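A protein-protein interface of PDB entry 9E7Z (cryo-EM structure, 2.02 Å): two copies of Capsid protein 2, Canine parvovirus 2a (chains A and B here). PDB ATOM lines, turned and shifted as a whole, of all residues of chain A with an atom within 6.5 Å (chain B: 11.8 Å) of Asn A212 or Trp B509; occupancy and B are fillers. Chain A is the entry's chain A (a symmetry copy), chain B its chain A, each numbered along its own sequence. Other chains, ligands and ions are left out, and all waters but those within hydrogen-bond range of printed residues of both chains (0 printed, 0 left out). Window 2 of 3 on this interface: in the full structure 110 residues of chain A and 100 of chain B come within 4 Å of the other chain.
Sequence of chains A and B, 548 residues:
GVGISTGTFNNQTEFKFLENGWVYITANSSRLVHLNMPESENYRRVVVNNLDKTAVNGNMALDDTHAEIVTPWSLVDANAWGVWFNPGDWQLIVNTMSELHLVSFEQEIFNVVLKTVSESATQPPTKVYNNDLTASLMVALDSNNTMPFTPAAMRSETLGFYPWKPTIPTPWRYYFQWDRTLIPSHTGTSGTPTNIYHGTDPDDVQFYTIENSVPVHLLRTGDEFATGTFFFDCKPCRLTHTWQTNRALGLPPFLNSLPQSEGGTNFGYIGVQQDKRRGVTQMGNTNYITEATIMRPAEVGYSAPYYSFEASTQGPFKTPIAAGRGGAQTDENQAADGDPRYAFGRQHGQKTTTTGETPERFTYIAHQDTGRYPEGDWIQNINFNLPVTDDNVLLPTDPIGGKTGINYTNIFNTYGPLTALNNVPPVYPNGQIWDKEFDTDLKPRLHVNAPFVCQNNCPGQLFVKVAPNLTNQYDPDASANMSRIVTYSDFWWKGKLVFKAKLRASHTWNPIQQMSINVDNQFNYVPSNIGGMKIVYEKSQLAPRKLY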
ATOM      1  N   TYR A  43      -2.915  -9.919 -21.177  1.00  0.00           N
ATOM      2  CA  TYR A  43      -3.941  -9.123 -20.520  1.00  0.00           C
ATOM      3  C   TYR A  43      -3.455  -7.687 -20.367  1.00  0.00           C
ATOM      4  O   TYR A  43      -2.305  -7.441 -19.998  1.00  0.00           O
ATOM      5  CB  TYR A  43      -4.278  -9.710 -19.151  1.00  0.00           C
ATOM      6  CG  TYR A  43      -4.946 -11.061 -19.208  1.00  0.00           C
ATOM      7  CD1 TYR A  43      -4.197 -12.222 -19.331  1.00  0.00           C
ATOM      8  CD2 TYR A  43      -6.325 -11.177 -19.137  1.00  0.00           C
ATOM      9  CE1 TYR A  43      -4.801 -13.458 -19.385  1.00  0.00           C
ATOM     10  CE2 TYR A  43      -6.938 -12.408 -19.188  1.00  0.00           C
ATOM     11  CZ  TYR A  43      -6.172 -13.548 -19.312  1.00  0.00           C
ATOM     12  OH  TYR A  43      -6.778 -14.778 -19.363  1.00  0.00           O
ATOM     13  N   GLN A 206      -9.288  -6.626  -8.520  1.00  0.00           N
ATOM     14  CA  GLN A 206      -9.620  -8.002  -8.904  1.00  0.00           C
ATOM     15  C   GLN A 206      -9.133  -8.215 -10.336  1.00  0.00           C
ATOM     16  O   GLN A 206      -9.783  -7.789 -11.294  1.00  0.00           O
ATOM     17  CB  GLN A 206     -11.113  -8.269  -8.763  1.00  0.00           C
ATOM     18  CG  GLN A 206     -11.587  -8.397  -7.321  1.00  0.00           C
ATOM     19  CD  GLN A 206     -13.058  -8.750  -7.217  1.00  0.00           C
ATOM     20  OE1 GLN A 206     -13.901  -8.159  -7.890  1.00  0.00           O
ATOM     21  NE2 GLN A 206     -13.371  -9.732  -6.384  1.00  0.00           N
ATOM     22  N   PHE A 207      -7.983  -8.871 -10.475  1.00  0.00           N
ATOM     23  CA  PHE A 207      -7.426  -9.209 -11.785  1.00  0.00           C
ATOM     24  C   PHE A 207      -7.722 -10.677 -12.059  1.00  0.00           C
ATOM     25  O   PHE A 207      -7.090 -11.569 -11.490  1.00  0.00           O
ATOM     26  CB  PHE A 207      -5.930  -8.914 -11.829  1.00  0.00           C
ATOM     27  CG  PHE A 207      -5.232  -9.451 -13.053  1.00  0.00           C
ATOM     28  CD1 PHE A 207      -5.862  -9.459 -14.288  1.00  0.00           C
ATOM     29  CD2 PHE A 207      -3.940  -9.936 -12.967  1.00  0.00           C
ATOM     30  CE1 PHE A 207      -5.218  -9.952 -15.407  1.00  0.00           C
ATOM     31  CE2 PHE A 207      -3.291 -10.426 -14.082  1.00  0.00           C
ATOM     32  CZ  PHE A 207      -3.930 -10.434 -15.304  1.00  0.00           C
ATOM     33  N   TYR A 208      -8.692 -10.928 -12.932  1.00  0.00           N
ATOM     34  CA  TYR A 208      -9.064 -12.281 -13.315  1.00  0.00           C
ATOM     35  C   TYR A 208      -8.338 -12.692 -14.588  1.00  0.00           C
ATOM     36  O   TYR A 208      -8.180 -11.894 -15.516  1.00  0.00           O
ATOM     37  CB  TYR A 208     -10.570 -12.393 -13.543  1.00  0.00           C
ATOM     38  CG  TYR A 208     -11.422 -12.106 -12.334  1.00  0.00           C
ATOM     39  CD1 TYR A 208     -11.663 -13.086 -11.385  1.00  0.00           C
ATOM     40  CD2 TYR A 208     -12.008 -10.863 -12.157  1.00  0.00           C
ATOM     41  CE1 TYR A 208     -12.452 -12.833 -10.285  1.00  0.00           C
ATOM     42  CE2 TYR A 208     -12.797 -10.598 -11.062  1.00  0.00           C
ATOM     43  CZ  TYR A 208     -13.017 -11.586 -10.128  1.00  0.00           C
ATOM     44  OH  TYR A 208     -13.804 -11.330  -9.032  1.00  0.00           O
ATOM     45  N   THR A 209      -7.906 -13.946 -14.629  1.00  0.00           N
ATOM     46  CA  THR A 209      -7.404 -14.563 -15.845  1.00  0.00           C
ATOM     47  C   THR A 209      -8.155 -15.864 -16.078  1.00  0.00           C
ATOM     48  O   THR A 209      -8.508 -16.575 -15.131  1.00  0.00           O
ATOM     49  CB  THR A 209      -5.892 -14.839 -15.778  1.00  0.00           C
ATOM     50  OG1 THR A 209      -5.618 -15.785 -14.739  1.00  0.00           O
ATOM     51  CG2 THR A 209      -5.119 -13.559 -15.510  1.00  0.00           C
ATOM     52  N   ILE A 210      -8.412 -16.162 -17.351  1.00  0.00           N
ATOM     53  CA  ILE A 210      -9.082 -17.412 -17.696  1.00  0.00           C
ATOM     54  C   ILE A 210      -8.224 -18.599 -17.278  1.00  0.00           C
ATOM     55  O   ILE A 210      -8.713 -19.571 -16.693  1.00  0.00           O
ATOM     56  CB  ILE A 210      -9.393 -17.449 -19.204  1.00  0.00           C
ATOM     57  CG1 ILE A 210     -10.405 -16.358 -19.576  1.00  0.00           C
ATOM     58  CG2 ILE A 210      -9.884 -18.832 -19.617  1.00  0.00           C
ATOM     59  CD1 ILE A 210     -11.809 -16.597 -19.071  1.00  0.00           C
ATOM     60  N   GLU A 211      -6.924 -18.524 -17.561  1.00  0.00           N
ATOM     61  CA  GLU A 211      -6.047 -19.677 -17.391  1.00  0.00           C
ATOM     62  C   GLU A 211      -5.961 -20.123 -15.936  1.00  0.00           C
ATOM     63  O   GLU A 211      -5.821 -21.319 -15.667  1.00  0.00           O
ATOM     64  CB  GLU A 211      -4.655 -19.344 -17.929  1.00  0.00           C
ATOM     65  CG  GLU A 211      -4.606 -19.155 -19.439  1.00  0.00           C
ATOM     66  CD  GLU A 211      -5.038 -17.766 -19.882  1.00  0.00           C
ATOM     67  OE1 GLU A 211      -5.547 -16.996 -19.041  1.00  0.00           O
ATOM     68  OE2 GLU A 211      -4.869 -17.443 -21.075  1.00  0.00           O
ATOM     69  N   ASN A 212      -6.041 -19.185 -14.990  1.00  0.00           N
ATOM     70  CA  ASN A 212      -5.907 -19.531 -13.579  1.00  0.00           C
ATOM     71  C   ASN A 212      -7.211 -19.998 -12.947  1.00  0.00           C
ATOM     72  O   ASN A 212      -7.179 -20.547 -11.842  1.00  0.00           O
ATOM     73  CB  ASN A 212      -5.375 -18.332 -12.789  1.00  0.00           C
ATOM     74  CG  ASN A 212      -3.925 -18.035 -13.089  1.00  0.00           C
ATOM     75  OD1 ASN A 212      -3.614 -17.179 -13.915  1.00  0.00           O
ATOM     76  ND2 ASN A 212      -3.025 -18.737 -12.415  1.00  0.00           N
ATOM     77  N   SER A 213      -8.349 -19.807 -13.613  1.00  0.00           N
ATOM     78  CA  SER A 213      -9.647 -20.069 -13.003  1.00  0.00           C
ATOM     79  C   SER A 213     -10.470 -21.134 -13.706  1.00  0.00           C
ATOM     80  O   SER A 213     -11.338 -21.734 -13.071  1.00  0.00           O
ATOM     81  CB  SER A 213     -10.474 -18.778 -12.953  1.00  0.00           C
ATOM     82  OG  SER A 213      -9.737 -17.725 -12.360  1.00  0.00           O
ATOM     83  N   VAL A 214     -10.226 -21.395 -14.987  1.00  0.00           N
ATOM     84  CA  VAL A 214     -11.100 -22.263 -15.772  1.00  0.00           C
ATOM     85  C   VAL A 214     -10.277 -23.357 -16.444  1.00  0.00           C
ATOM     86  O   VAL A 214      -9.203 -23.069 -16.986  1.00  0.00           O
ATOM     87  CB  VAL A 214     -11.878 -21.455 -16.824  1.00  0.00           C
ATOM     88  CG1 VAL A 214     -12.960 -22.308 -17.465  1.00  0.00           C
ATOM     89  CG2 VAL A 214     -12.478 -20.199 -16.204  1.00  0.00           C
ATOM     90  N   ARG B 504     -12.043 -18.697   3.120  1.00  0.00           N
ATOM     91  CA  ARG B 504     -12.030 -17.986   1.850  1.00  0.00           C
ATOM     92  C   ARG B 504     -11.128 -18.689   0.841  1.00  0.00           C
ATOM     93  O   ARG B 504     -10.160 -19.365   1.197  1.00  0.00           O
ATOM     94  CB  ARG B 504     -11.563 -16.542   2.049  1.00  0.00           C
ATOM     95  CG  ARG B 504     -10.053 -16.355   2.115  1.00  0.00           C
ATOM     96  CD  ARG B 504      -9.674 -14.886   2.195  1.00  0.00           C
ATOM     97  NE  ARG B 504      -8.230 -14.700   2.237  1.00  0.00           N
ATOM     98  CZ  ARG B 504      -7.438 -14.679   1.173  1.00  0.00           C
ATOM     99  NH1 ARG B 504      -7.920 -14.808  -0.052  1.00  0.00           N
ATOM    100  NH2 ARG B 504      -6.129 -14.522   1.342  1.00  0.00           N
ATOM    101  N   ALA B 505     -11.456 -18.515  -0.432  1.00  0.00           N
ATOM    102  CA  ALA B 505     -10.637 -18.987  -1.537  1.00  0.00           C
ATOM    103  C   ALA B 505     -10.021 -17.800  -2.271  1.00  0.00           C
ATOM    104  O   ALA B 505     -10.528 -16.678  -2.224  1.00  0.00           O
ATOM    105  CB  ALA B 505     -11.466 -19.832  -2.507  1.00  0.00           C
ATOM    106  N   SER B 506      -8.908 -18.063  -2.950  1.00  0.00           N
ATOM    107  CA  SER B 506      -8.222 -17.050  -3.746  1.00  0.00           C
ATOM    108  C   SER B 506      -8.749 -17.127  -5.175  1.00  0.00           C
ATOM    109  O   SER B 506      -8.496 -18.102  -5.886  1.00  0.00           O
ATOM    110  CB  SER B 506      -6.711 -17.260  -3.703  1.00  0.00           C
ATOM    111  OG  SER B 506      -6.036 -16.233  -4.405  1.00  0.00           O
ATOM    112  N   HIS B 507      -9.479 -16.097  -5.594  1.00  0.00           N
ATOM    113  CA  HIS B 507     -10.129 -16.089  -6.897  1.00  0.00           C
ATOM    114  C   HIS B 507      -9.330 -15.365  -7.972  1.00  0.00           C
ATOM    115  O   HIS B 507      -9.619 -15.549  -9.158  1.00  0.00           O
ATOM    116  CB  HIS B 507     -11.511 -15.430  -6.795  1.00  0.00           C
ATOM    117  CG  HIS B 507     -12.329 -15.905  -5.636  1.00  0.00           C
ATOM    118  ND1 HIS B 507     -13.099 -17.047  -5.686  1.00  0.00           N
ATOM    119  CD2 HIS B 507     -12.505 -15.386  -4.399  1.00  0.00           C
ATOM    120  CE1 HIS B 507     -13.710 -17.213  -4.527  1.00  0.00           C
ATOM    121  NE2 HIS B 507     -13.366 -16.219  -3.728  1.00  0.00           N
ATOM    122  N   THR B 508      -8.346 -14.551  -7.599  1.00  0.00           N
ATOM    123  CA  THR B 508      -7.699 -13.646  -8.535  1.00  0.00           C
ATOM    124  C   THR B 508      -6.190 -13.843  -8.515  1.00  0.00           C
ATOM    125  O   THR B 508      -5.622 -14.419  -7.586  1.00  0.00           O
ATOM    126  CB  THR B 508      -8.029 -12.176  -8.218  1.00  0.00           C
ATOM    127  OG1 THR B 508      -7.646 -11.872  -6.870  1.00  0.00           O
ATOM    128  CG2 THR B 508      -9.517 -11.907  -8.399  1.00  0.00           C
ATOM    129  N   TRP B 509      -5.553 -13.347  -9.576  1.00  0.00           N
ATOM    130  CA  TRP B 509      -4.097 -13.341  -9.649  1.00  0.00           C
ATOM    131  C   TRP B 509      -3.495 -12.523  -8.513  1.00  0.00           C
ATOM    132  O   TRP B 509      -2.528 -12.945  -7.871  1.00  0.00           O
ATOM    133  CB  TRP B 509      -3.658 -12.783 -11.004  1.00  0.00           C
ATOM    134  CG  TRP B 509      -2.176 -12.653 -11.158  1.00  0.00           C
ATOM    135  CD1 TRP B 509      -1.404 -11.594 -10.787  1.00  0.00           C
ATOM    136  CD2 TRP B 509      -1.289 -13.617 -11.731  1.00  0.00           C
ATOM    137  NE1 TRP B 509      -0.088 -11.840 -11.089  1.00  0.00           N
ATOM    138  CE2 TRP B 509       0.010 -13.076 -11.669  1.00  0.00           C
ATOM    139  CE3 TRP B 509      -1.464 -14.886 -12.289  1.00  0.00           C
ATOM    140  CZ2 TRP B 509       1.127 -13.760 -12.143  1.00  0.00           C
ATOM    141  CZ3 TRP B 509      -0.355 -15.563 -12.757  1.00  0.00           C
ATOM    142  CH2 TRP B 509       0.925 -14.999 -12.681  1.00  0.00           C
ATOM    143  N   ASN B 510      -4.060 -11.348  -8.253  1.00  0.00           N
ATOM    144  CA  ASN B 510      -3.491 -10.429  -7.281  1.00  0.00           C
ATOM    145  C   ASN B 510      -3.810 -10.874  -5.854  1.00  0.00           C
ATOM    146  O   ASN B 510      -4.782 -11.593  -5.620  1.00  0.00           O
ATOM    147  CB  ASN B 510      -4.037  -9.021  -7.497  1.00  0.00           C
ATOM    148  CG  ASN B 510      -5.554  -8.967  -7.417  1.00  0.00           C
ATOM    149  OD1 ASN B 510      -6.245  -9.285  -8.379  1.00  0.00           O
ATOM    150  ND2 ASN B 510      -6.074  -8.577  -6.262  1.00  0.00           N
ATOM    151  N   PRO B 511      -3.006 -10.452  -4.881  1.00  0.00           N
ATOM    152  CA  PRO B 511      -3.402 -10.609  -3.480  1.00  0.00           C
ATOM    153  C   PRO B 511      -4.471  -9.595  -3.100  1.00  0.00           C
ATOM    154  O   PRO B 511      -4.729  -8.623  -3.813  1.00  0.00           O
ATOM    155  CB  PRO B 511      -2.100 -10.366  -2.712  1.00  0.00           C
ATOM    156  CG  PRO B 511      -1.317  -9.465  -3.599  1.00  0.00           C
ATOM    157  CD  PRO B 511      -1.668  -9.846  -5.009  1.00  0.00           C
ATOM    158  N   ILE B 512      -5.098  -9.837  -1.956  1.00  0.00           N
ATOM    159  CA  ILE B 512      -6.175  -8.995  -1.468  1.00  0.00           C
ATOM    160  C   ILE B 512      -5.724  -8.280  -0.200  1.00  0.00           C
ATOM    161  O   ILE B 512      -4.679  -8.575   0.372  1.00  0.00           O
ATOM    162  CB  ILE B 512      -7.467  -9.806  -1.211  1.00  0.00           C
ATOM    163  CG1 ILE B 512      -7.166 -10.994  -0.291  1.00  0.00           C
ATOM    164  CG2 ILE B 512      -8.076 -10.265  -2.529  1.00  0.00           C
ATOM    165  CD1 ILE B 512      -8.217 -11.248   0.747  1.00  0.00           C
ATOM    166  N   GLN B 513      -6.535  -7.326   0.253  1.00  0.00           N
ATOM    167  CA  GLN B 513      -6.253  -6.625   1.496  1.00  0.00           C
ATOM    168  C   GLN B 513      -6.365  -7.576   2.682  1.00  0.00           C
ATOM    169  O   GLN B 513      -7.240  -8.443   2.723  1.00  0.00           O
ATOM    170  CB  GLN B 513      -7.219  -5.451   1.664  1.00  0.00           C
ATOM    171  CG  GLN B 513      -7.212  -4.820   3.048  1.00  0.00           C
ATOM    172  CD  GLN B 513      -8.180  -3.661   3.162  1.00  0.00           C
ATOM    173  OE1 GLN B 513      -9.395  -3.839   3.075  1.00  0.00           O
ATOM    174  NE2 GLN B 513      -7.643  -2.464   3.359  1.00  0.00           N
ATOM    175  N   PRO B 544     -12.445  -8.274  -1.330  1.00  0.00           N
ATOM    176  CA  PRO B 544     -13.535  -7.949  -2.253  1.00  0.00           C
ATOM    177  C   PRO B 544     -14.246  -9.203  -2.731  1.00  0.00           C
ATOM    178  O   PRO B 544     -13.729 -10.318  -2.656  1.00  0.00           O
ATOM    179  CB  PRO B 544     -12.818  -7.246  -3.407  1.00  0.00           C
ATOM    180  CG  PRO B 544     -11.472  -7.878  -3.428  1.00  0.00           C
ATOM    181  CD  PRO B 544     -11.131  -8.201  -1.994  1.00  0.00           C
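The backbone NH of Trp B509 is in hydrogen-bond range of the backbone carbonyl oxygen of Phe A207, at 3.0 Å.
The backbone NH (N) of Phe A207 sits at hydrogen-bond distance from the side-chain amide oxygen (OD1) of Asn B510, at 2.8 Å.
The side-chain amide oxygen (OD1) of Asn A212 lies within hydrogen-bond range of the side-chain hydroxyl (OG1) of Thr A209, at 2.6 Å.
The side-chain hydroxyl (OG) of Ser A213 lies within hydrogen-bond range of the backbone carbonyl oxygen (O) of Thr A209 (3.2 Å).
The side-chain hydroxyl (OH) of Tyr A208 lies within hydrogen-bond range of the side-chain amide nitrogen (NE2) of Gln A206 (3.1 Å).
A ring nitrogen (NE2) of His B507 lies close to the backbone carbonyl oxygen (O) of Ala B505 (3.2 Å).
The side-chain hydroxyl (OG1) of Thr B508 lies within hydrogen-bond range of the backbone carbonyl oxygen (O) of Asn B510 (3.1 Å).
CA of Gln A206 touches CG2 of Thr B508, at 3.9 Å.
CA of Gln A206 touches OD1 of Asn B510, at 3.6 Å.
NE2 of Gln A206 touches O of Pro B544, at 3.8 Å.
Phe A207 touches Thr B508 (O to CB, 3.5 Å).
Tyr A208 touches His B507 (CD1 to O, 3.9 Å).
Thr B508 touches Tyr A208.
Trp B509 touches Asn A212 (CE3 to OD1, 3.5 Å).
Ser A213 touches His B507 (OG to O, 3.9 Å).
Asn A212 touches just one residue of chain B: Trp B509 (3.5 Å).
Of chain A, only Phe A207 and Asn A212 come within 4 Å of Trp B509.
Phe A207 touches three residues of chain B.
No residue of chain B comes within 4 Å of Thr A209.
No residue of chain B comes within 4 Å of Ile A210.
No residue of chain B comes within 4 Å of Glu A211.
Of chain B, only His B507 comes within 4 Å of Ser A213.
Val A214 touches none of the printed residues of chain B.
Of the printed residues of chain A, His B507 touches Tyr A208 and Ser A213.
Printed residues of chain A within 4 Å of Thr B508: Gln A206 (3.9 Å), Phe A207 (3.5 Å) and Tyr A208 (3.6 Å).
Of the printed residues of chain B, Tyr A208 touches His B507 and Thr B508.
Ile B512 touches none of the printed residues of chain A.
Ala B505 touches none of the printed residues of chain A.
The nearest residue of chain B that does not touch Asn A212 is His B507 (6.2 Å).
The nearest residue of chain A that does not touch Trp B509 is Thr A209 (4.8 Å).
Among the printed residues, no Asp or Glu carboxylate lies within 4 Å of a Lys or Arg side-chain nitrogen of the other chain.
No position is printed for both chains.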
